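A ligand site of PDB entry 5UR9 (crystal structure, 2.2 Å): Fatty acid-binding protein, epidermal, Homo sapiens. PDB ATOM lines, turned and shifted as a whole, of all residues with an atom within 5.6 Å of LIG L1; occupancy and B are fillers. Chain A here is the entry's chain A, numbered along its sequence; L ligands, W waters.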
ATOM      1  N   LEU A  16      19.599 -23.441   3.076  1.00  0.00           N
ATOM      2  CA  LEU A  16      18.596 -23.086   4.088  1.00  0.00           C
ATOM      3  C   LEU A  16      18.033 -24.341   4.749  1.00  0.00           C
ATOM      4  O   LEU A  16      17.539 -25.252   4.064  1.00  0.00           O
ATOM      5  CB  LEU A  16      17.461 -22.293   3.454  1.00  0.00           C
ATOM      6  CG  LEU A  16      16.413 -21.837   4.480  1.00  0.00           C
ATOM      7  CD1 LEU A  16      16.988 -20.746   5.391  1.00  0.00           C
ATOM      8  CD2 LEU A  16      15.125 -21.358   3.797  1.00  0.00           C
ATOM      9  N   PHE A  22       9.786 -15.194   8.533  1.00  0.00           N
ATOM     10  CA  PHE A  22      10.132 -14.585   7.260  1.00  0.00           C
ATOM     11  C   PHE A  22       8.930 -13.901   6.635  1.00  0.00           C
ATOM     12  O   PHE A  22       9.062 -12.817   6.064  1.00  0.00           O
ATOM     13  CB  PHE A  22      10.761 -15.623   6.333  1.00  0.00           C
ATOM     14  CG  PHE A  22      11.416 -15.030   5.116  1.00  0.00           C
ATOM     15  CD1 PHE A  22      12.257 -13.920   5.227  1.00  0.00           C
ATOM     16  CD2 PHE A  22      11.243 -15.622   3.856  1.00  0.00           C
ATOM     17  CE1 PHE A  22      12.876 -13.389   4.109  1.00  0.00           C
ATOM     18  CE2 PHE A  22      11.866 -15.101   2.731  1.00  0.00           C
ATOM     19  CZ  PHE A  22      12.699 -13.980   2.859  1.00  0.00           C
ATOM     20  N   TYR A  25       8.435 -10.638   8.327  1.00  0.00           N
ATOM     21  CA  TYR A  25       9.464  -9.683   7.941  1.00  0.00           C
ATOM     22  C   TYR A  25       9.176  -9.111   6.552  1.00  0.00           C
ATOM     23  O   TYR A  25       9.178  -7.883   6.363  1.00  0.00           O
ATOM     24  CB  TYR A  25      10.847 -10.355   8.026  1.00  0.00           C
ATOM     25  CG  TYR A  25      11.940  -9.507   7.456  1.00  0.00           C
ATOM     26  CD1 TYR A  25      12.341  -8.348   8.105  1.00  0.00           C
ATOM     27  CD2 TYR A  25      12.577  -9.866   6.259  1.00  0.00           C
ATOM     28  CE1 TYR A  25      13.344  -7.555   7.585  1.00  0.00           C
ATOM     29  CE2 TYR A  25      13.593  -9.094   5.736  1.00  0.00           C
ATOM     30  CZ  TYR A  25      13.963  -7.933   6.403  1.00  0.00           C
ATOM     31  OH  TYR A  25      14.957  -7.139   5.901  1.00  0.00           O
ATOM     32  N   MET A  26       8.867  -9.967   5.584  1.00  0.00           N
ATOM     33  CA  MET A  26       8.542  -9.470   4.251  1.00  0.00           C
ATOM     34  C   MET A  26       7.321  -8.567   4.294  1.00  0.00           C
ATOM     35  O   MET A  26       7.283  -7.510   3.640  1.00  0.00           O
ATOM     36  CB  MET A  26       8.339 -10.647   3.299  1.00  0.00           C
ATOM     37  CG  MET A  26       9.634 -11.324   2.868  1.00  0.00           C
ATOM     38  SD  MET A  26       9.256 -12.612   1.670  1.00  0.00           S
ATOM     39  CE  MET A  26       8.322 -13.773   2.685  1.00  0.00           C
ATOM     40  N   LEU A  29       8.353  -5.281   5.194  1.00  0.00           N
ATOM     41  CA  LEU A  29       9.004  -4.610   4.068  1.00  0.00           C
ATOM     42  C   LEU A  29       8.026  -4.084   3.032  1.00  0.00           C
ATOM     43  O   LEU A  29       8.452  -3.341   2.146  1.00  0.00           O
ATOM     44  CB  LEU A  29       9.990  -5.533   3.335  1.00  0.00           C
ATOM     45  CG  LEU A  29      11.306  -5.944   3.981  1.00  0.00           C
ATOM     46  CD1 LEU A  29      11.938  -7.035   3.140  1.00  0.00           C
ATOM     47  CD2 LEU A  29      12.228  -4.743   4.102  1.00  0.00           C
ATOM     48  N   VAL A  31       6.108  -6.235   1.065  1.00  0.00           N
ATOM     49  CA  VAL A  31       6.062  -7.213  -0.017  1.00  0.00           C
ATOM     50  C   VAL A  31       4.642  -7.738  -0.136  1.00  0.00           C
ATOM     51  O   VAL A  31       4.003  -8.058   0.873  1.00  0.00           O
ATOM     52  CB  VAL A  31       7.044  -8.358   0.257  1.00  0.00           C
ATOM     53  CG1 VAL A  31       6.998  -9.380  -0.865  1.00  0.00           C
ATOM     54  CG2 VAL A  31       8.459  -7.824   0.475  1.00  0.00           C
ATOM     55  N   LEU A  35       4.538 -12.475  -3.662  1.00  0.00           N
ATOM     56  CA  LEU A  35       5.977 -12.577  -3.487  1.00  0.00           C
ATOM     57  C   LEU A  35       6.305 -13.202  -2.130  1.00  0.00           C
ATOM     58  O   LEU A  35       7.245 -13.982  -2.045  1.00  0.00           O
ATOM     59  CB  LEU A  35       6.641 -11.209  -3.646  1.00  0.00           C
ATOM     60  CG  LEU A  35       8.167 -11.165  -3.745  1.00  0.00           C
ATOM     61  CD1 LEU A  35       8.693 -12.084  -4.812  1.00  0.00           C
ATOM     62  CD2 LEU A  35       8.635  -9.746  -4.029  1.00  0.00           C
ATOM     63  N   GLY A  39       8.619 -16.395  -1.784  1.00  0.00           N
ATOM     64  CA  GLY A  39       9.806 -16.317  -0.944  1.00  0.00           C
ATOM     65  C   GLY A  39       9.789 -17.343   0.174  1.00  0.00           C
ATOM     66  O   GLY A  39      10.805 -17.965   0.474  1.00  0.00           O
ATOM     67  N   ALA A  42      10.667 -20.817  -1.260  1.00  0.00           N
ATOM     68  CA  ALA A  42      12.014 -21.028  -1.763  1.00  0.00           C
ATOM     69  C   ALA A  42      12.920 -21.599  -0.669  1.00  0.00           C
ATOM     70  O   ALA A  42      12.748 -21.363   0.526  1.00  0.00           O
ATOM     71  CB  ALA A  42      12.586 -19.714  -2.312  1.00  0.00           C
ATOM     72  N   PRO A  44      16.620 -21.385  -0.763  1.00  0.00           N
ATOM     73  CA  PRO A  44      17.774 -20.926  -1.536  1.00  0.00           C
ATOM     74  C   PRO A  44      19.085 -21.213  -0.847  1.00  0.00           C
ATOM     75  O   PRO A  44      19.185 -21.146   0.377  1.00  0.00           O
ATOM     76  CB  PRO A  44      17.553 -19.398  -1.639  1.00  0.00           C
ATOM     77  CG  PRO A  44      16.211 -19.138  -1.037  1.00  0.00           C
ATOM     78  CD  PRO A  44      15.921 -20.279  -0.103  1.00  0.00           C
ATOM     79  N   CYS A  46      22.793 -19.778  -0.182  1.00  0.00           N
ATOM     80  CA  CYS A  46      23.447 -18.484  -0.047  1.00  0.00           C
ATOM     81  C   CYS A  46      24.940 -18.715  -0.193  1.00  0.00           C
ATOM     82  O   CYS A  46      25.506 -19.572   0.486  1.00  0.00           O
ATOM     83  CB  CYS A  46      23.097 -17.853   1.293  1.00  0.00           C
ATOM     84  SG  CYS A  46      24.010 -16.326   1.696  1.00  0.00           S
ATOM     85  N   THR A  59      22.262 -15.271  -3.758  1.00  0.00           N
ATOM     86  CA  THR A  59      21.112 -16.062  -3.346  1.00  0.00           C
ATOM     87  C   THR A  59      20.611 -16.829  -4.564  1.00  0.00           C
ATOM     88  O   THR A  59      20.237 -16.224  -5.583  1.00  0.00           O
ATOM     89  CB  THR A  59      20.050 -15.141  -2.752  1.00  0.00           C
ATOM     90  OG1 THR A  59      20.645 -14.321  -1.726  1.00  0.00           O
ATOM     91  CG2 THR A  59      18.877 -15.921  -2.206  1.00  0.00           C
ATOM     92  N   ALA A  81      15.423  -8.014  -4.037  1.00  0.00           N
ATOM     93  CA  ALA A  81      14.580  -8.920  -4.808  1.00  0.00           C
ATOM     94  C   ALA A  81      13.152  -8.428  -4.878  1.00  0.00           C
ATOM     95  O   ALA A  81      12.470  -8.614  -5.891  1.00  0.00           O
ATOM     96  CB  ALA A  81      14.634 -10.335  -4.226  1.00  0.00           C
ATOM     97  N   ASP A  82      12.664  -7.808  -3.798  1.00  0.00           N
ATOM     98  CA  ASP A  82      11.325  -7.242  -3.829  1.00  0.00           C
ATOM     99  C   ASP A  82      11.275  -5.912  -4.570  1.00  0.00           C
ATOM    100  O   ASP A  82      10.187  -5.369  -4.742  1.00  0.00           O
ATOM    101  CB  ASP A  82      10.771  -7.054  -2.406  1.00  0.00           C
ATOM    102  CG  ASP A  82      11.698  -6.237  -1.505  1.00  0.00           C
ATOM    103  OD1 ASP A  82      12.917  -6.514  -1.504  1.00  0.00           O
ATOM    104  OD2 ASP A  82      11.225  -5.329  -0.792  1.00  0.00           O
ATOM    105  N   ARG A  84      13.219  -2.895  -3.949  1.00  0.00           N
ATOM    106  CA  ARG A  84      13.639  -1.666  -3.297  1.00  0.00           C
ATOM    107  C   ARG A  84      15.002  -1.246  -3.815  1.00  0.00           C
ATOM    108  O   ARG A  84      15.849  -2.082  -4.144  1.00  0.00           O
ATOM    109  CB  ARG A  84      13.686  -1.863  -1.772  1.00  0.00           C
ATOM    110  CG  ARG A  84      12.306  -1.991  -1.131  1.00  0.00           C
ATOM    111  CD  ARG A  84      12.366  -2.508   0.306  1.00  0.00           C
ATOM    112  NE  ARG A  84      12.861  -3.880   0.365  1.00  0.00           N
ATOM    113  CZ  ARG A  84      13.917  -4.254   1.079  1.00  0.00           C
ATOM    114  NH1 ARG A  84      14.567  -3.358   1.832  1.00  0.00           N
ATOM    115  NH2 ARG A  84      14.309  -5.524   1.043  1.00  0.00           N
ATOM    116  N   ILE A 110      20.160  -6.830   8.335  1.00  0.00           N
ATOM    117  CA  ILE A 110      20.311  -8.279   8.193  1.00  0.00           C
ATOM    118  C   ILE A 110      21.667  -8.654   8.800  1.00  0.00           C
ATOM    119  O   ILE A 110      22.717  -8.221   8.303  1.00  0.00           O
ATOM    120  CB  ILE A 110      20.224  -8.738   6.729  1.00  0.00           C
ATOM    121  CG1 ILE A 110      18.895  -8.314   6.109  1.00  0.00           C
ATOM    122  CG2 ILE A 110      20.396 -10.255   6.616  1.00  0.00           C
ATOM    123  CD1 ILE A 110      18.800  -8.565   4.623  1.00  0.00           C
ATOM    124  N   ARG A 112      24.346 -11.712   9.902  1.00  0.00           N
ATOM    125  CA  ARG A 112      24.729 -13.094   9.625  1.00  0.00           C
ATOM    126  C   ARG A 112      25.923 -13.454  10.508  1.00  0.00           C
ATOM    127  O   ARG A 112      26.977 -12.803  10.432  1.00  0.00           O
ATOM    128  CB  ARG A 112      25.077 -13.276   8.143  1.00  0.00           C
ATOM    129  CG  ARG A 112      23.946 -12.943   7.181  1.00  0.00           C
ATOM    130  CD  ARG A 112      24.424 -13.061   5.747  1.00  0.00           C
ATOM    131  NE  ARG A 112      23.378 -12.792   4.755  1.00  0.00           N
ATOM    132  CZ  ARG A 112      23.170 -11.571   4.248  1.00  0.00           C
ATOM    133  NH1 ARG A 112      23.916 -10.536   4.644  1.00  0.00           N
ATOM    134  NH2 ARG A 112      22.226 -11.374   3.348  1.00  0.00           N
ATOM    135  N   VAL A 121      21.023 -16.149  10.287  1.00  0.00           N
ATOM    136  CA  VAL A 121      20.705 -14.927   9.555  1.00  0.00           C
ATOM    137  C   VAL A 121      19.453 -14.353  10.197  1.00  0.00           C
ATOM    138  O   VAL A 121      18.391 -14.974  10.154  1.00  0.00           O
ATOM    139  CB  VAL A 121      20.453 -15.217   8.071  1.00  0.00           C
ATOM    140  CG1 VAL A 121      20.167 -13.927   7.315  1.00  0.00           C
ATOM    141  CG2 VAL A 121      21.623 -15.970   7.449  1.00  0.00           C
ATOM    142  N   CYS A 123      16.896 -11.122  10.265  1.00  0.00           N
ATOM    143  CA  CYS A 123      16.448  -9.950   9.528  1.00  0.00           C
ATOM    144  C   CYS A 123      15.496  -9.165  10.403  1.00  0.00           C
ATOM    145  O   CYS A 123      14.531  -9.715  10.943  1.00  0.00           O
ATOM    146  CB  CYS A 123      15.771 -10.333   8.208  1.00  0.00           C
ATOM    147  SG  CYS A 123      16.627 -11.592   7.293  1.00  0.00           S
ATOM    148  N   ARG A 132      16.712 -17.236  10.128  1.00  0.00           N
ATOM    149  CA  ARG A 132      16.894 -18.260   9.110  1.00  0.00           C
ATOM    150  C   ARG A 132      18.236 -18.929   9.343  1.00  0.00           C
ATOM    151  O   ARG A 132      19.231 -18.264   9.651  1.00  0.00           O
ATOM    152  CB  ARG A 132      16.789 -17.650   7.709  1.00  0.00           C
ATOM    153  CG  ARG A 132      15.343 -17.299   7.396  1.00  0.00           C
ATOM    154  CD  ARG A 132      15.213 -16.216   6.344  1.00  0.00           C
ATOM    155  NE  ARG A 132      15.510 -16.668   4.984  1.00  0.00           N
ATOM    156  CZ  ARG A 132      14.713 -17.452   4.247  1.00  0.00           C
ATOM    157  NH1 ARG A 132      13.573 -17.914   4.747  1.00  0.00           N
ATOM    158  NH2 ARG A 132      15.055 -17.763   3.009  1.00  0.00           N
ATOM    159  N   TYR A 134      21.125 -21.751   8.000  1.00  0.00           N
ATOM    160  CA  TYR A 134      21.734 -22.464   6.889  1.00  0.00           C
ATOM    161  C   TYR A 134      22.850 -23.372   7.366  1.00  0.00           C
ATOM    162  O   TYR A 134      23.623 -23.025   8.276  1.00  0.00           O
ATOM    163  CB  TYR A 134      22.341 -21.536   5.830  1.00  0.00           C
ATOM    164  CG  TYR A 134      21.395 -20.590   5.120  1.00  0.00           C
ATOM    165  CD1 TYR A 134      20.839 -19.485   5.785  1.00  0.00           C
ATOM    166  CD2 TYR A 134      21.108 -20.748   3.764  1.00  0.00           C
ATOM    167  CE1 TYR A 134      20.004 -18.595   5.125  1.00  0.00           C
ATOM    168  CE2 TYR A 134      20.269 -19.849   3.090  1.00  0.00           C
ATOM    169  CZ  TYR A 134      19.721 -18.782   3.785  1.00  0.00           C
ATOM    170  OH  TYR A 134      18.882 -17.881   3.133  1.00  0.00           O
HETATM  171  C1  LIG L   1      18.195 -14.306   3.801  1.00  0.00           C
HETATM  172  O1  LIG L   1      19.368 -14.390   3.367  1.00  0.00           O
HETATM  173  O2  LIG L   1      17.666 -15.382   4.091  1.00  0.00           O
HETATM  174  C2  LIG L   1      17.449 -12.990   4.002  1.00  0.00           C
HETATM  175  C3  LIG L   1      17.345 -12.083   2.777  1.00  0.00           C
HETATM  176  C4  LIG L   1      15.921 -11.905   2.210  1.00  0.00           C
HETATM  177  C5  LIG L   1      15.310 -10.515   2.450  1.00  0.00           C
HETATM  178  C6  LIG L   1      14.606  -9.885   1.239  1.00  0.00           C
HETATM  179  C7  LIG L   1      13.142 -10.265   1.174  1.00  0.00           C
HETATM  180  C8  LIG L   1      12.499  -9.979  -0.178  1.00  0.00           C
HETATM  181  C9  LIG L   1      11.399 -10.996  -0.496  1.00  0.00           C
HETATM  182  C10 LIG L   1      11.673 -11.725  -1.809  1.00  0.00           C
HETATM  183  C11 LIG L   1      12.921 -12.621  -1.772  1.00  0.00           C
HETATM  184  C12 LIG L   1      12.649 -13.966  -1.102  1.00  0.00           C
HETATM  185  C13 LIG L   1      13.928 -14.540  -0.482  1.00  0.00           C
HETATM  186  C14 LIG L   1      14.980 -14.868  -1.528  1.00  0.00           C
HETATM  187  C1  LG2 L   2      11.218 -11.559  -7.495  1.00  0.00           C
HETATM  188  C2  LG2 L   2      14.669 -10.707  -8.570  1.00  0.00           C
HETATM  189  C3  LG2 L   2      15.982 -11.132  -8.767  1.00  0.00           C
HETATM  190  O1  LG2 L   2      12.355 -13.021  -5.900  1.00  0.00           O
HETATM  191  C4  LG2 L   2      12.742 -14.271  -5.479  1.00  0.00           C
HETATM  192  O2  LG2 L   2       9.911 -10.751 -11.623  1.00  0.00           O
HETATM  193  C5  LG2 L   2      10.760 -10.429 -10.774  1.00  0.00           C
HETATM  194  O3  LG2 L   2      11.404  -9.369 -10.780  1.00  0.00           O
HETATM  195  C6  LG2 L   2      11.042 -11.415  -9.632  1.00  0.00           C
HETATM  196  C7  LG2 L   2      12.146 -10.931  -8.634  1.00  0.00           C
HETATM  197  C8  LG2 L   2      13.535 -11.472  -8.883  1.00  0.00           C
HETATM  198  C9  LG2 L   2      13.799 -12.727  -9.446  1.00  0.00           C
HETATM  199  C10 LG2 L   2      15.130 -13.173  -9.654  1.00  0.00           C
HETATM  200  C11 LG2 L   2      16.224 -12.367  -9.331  1.00  0.00           C
HETATM  201  C12 LG2 L   2      11.550 -12.895  -7.026  1.00  0.00           C
HETATM  202  O4  LG2 L   2      11.400 -13.919  -7.718  1.00  0.00           O
HETATM  203  C13 LG2 L   2      11.832 -15.194  -4.956  1.00  0.00           C
HETATM  204  C14 LG2 L   2      12.254 -16.462  -4.516  1.00  0.00           C
HETATM  205  C15 LG2 L   2      13.563 -16.827  -4.597  1.00  0.00           C
HETATM  206  C16 LG2 L   2      14.540 -15.906  -5.142  1.00  0.00           C
HETATM  207  C17 LG2 L   2      15.911 -16.263  -5.237  1.00  0.00           C
HETATM  208  C18 LG2 L   2      16.861 -15.428  -5.743  1.00  0.00           C
HETATM  209  C19 LG2 L   2      16.479 -14.149  -6.175  1.00  0.00           C
HETATM  210  C20 LG2 L   2      15.166 -13.766  -6.109  1.00  0.00           C
HETATM  211  C21 LG2 L   2      14.140 -14.628  -5.583  1.00  0.00           C
HETATM  212  C22 LG2 L   2       9.992 -11.386  -8.456  1.00  0.00           C
HETATM  213  C23 LG2 L   2       9.219 -10.147  -8.217  1.00  0.00           C
HETATM  214  C24 LG2 L   2       7.834 -10.053  -8.476  1.00  0.00           C
HETATM  215  C25 LG2 L   2       7.141  -8.864  -8.237  1.00  0.00           C
HETATM  216  C26 LG2 L   2       7.797  -7.727  -7.715  1.00  0.00           C
HETATM  217  C27 LG2 L   2       9.160  -7.799  -7.436  1.00  0.00           C
HETATM  218  C28 LG2 L   2       9.826  -8.989  -7.689  1.00  0.00           C
HETATM  219  O   HOH W   1      22.062 -15.243   4.087  1.00  0.00           O
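Water W1 lies within hydrogen-bond range of NE of Arg 112 (2.9 Å), O1 of LIG L1 (2.9 Å) and SG of Cys 46 (3.3 Å).
The backbone NH (N) of Arg 132 is in hydrogen-bond range of the backbone carbonyl oxygen (O) of Val 121, at 2.8 Å.
The backbone NH (N) of Val 31 is in hydrogen-bond range of the backbone carbonyl oxygen (O) of Met 26 (3.1 Å).
The guanidinium group of Arg 84 is in salt-bridge range of the side-chain carboxylate of Asp 82 (2.5 Å).
Phe 22 touches LIG L1 (CZ to C13, 3.6 Å).
Tyr 25 touches LIG L1 (CE2 to C5, 3.97 Å).
SD of Met 26 touches C9 of LIG L1 (3.4 Å).
Leu 29 touches LIG L1.
Gly 39 touches LIG L1.
Ala 81 touches LIG L1 (CB to C11, 3.8 Å).
Asp 82 touches LIG L1 (OD1 to C8, 3.7 Å).
SG of Cys 123 touches C2 of LIG L1, 3.7 Å away.
O2 of LIG L1 lies within salt-bridge range of NE of Arg 132, 2.7 Å away.
The side-chain hydroxyl (OH) of Tyr 134 is in hydrogen-bond range of an oxygen (O2) of LIG L1 (2.9 Å).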
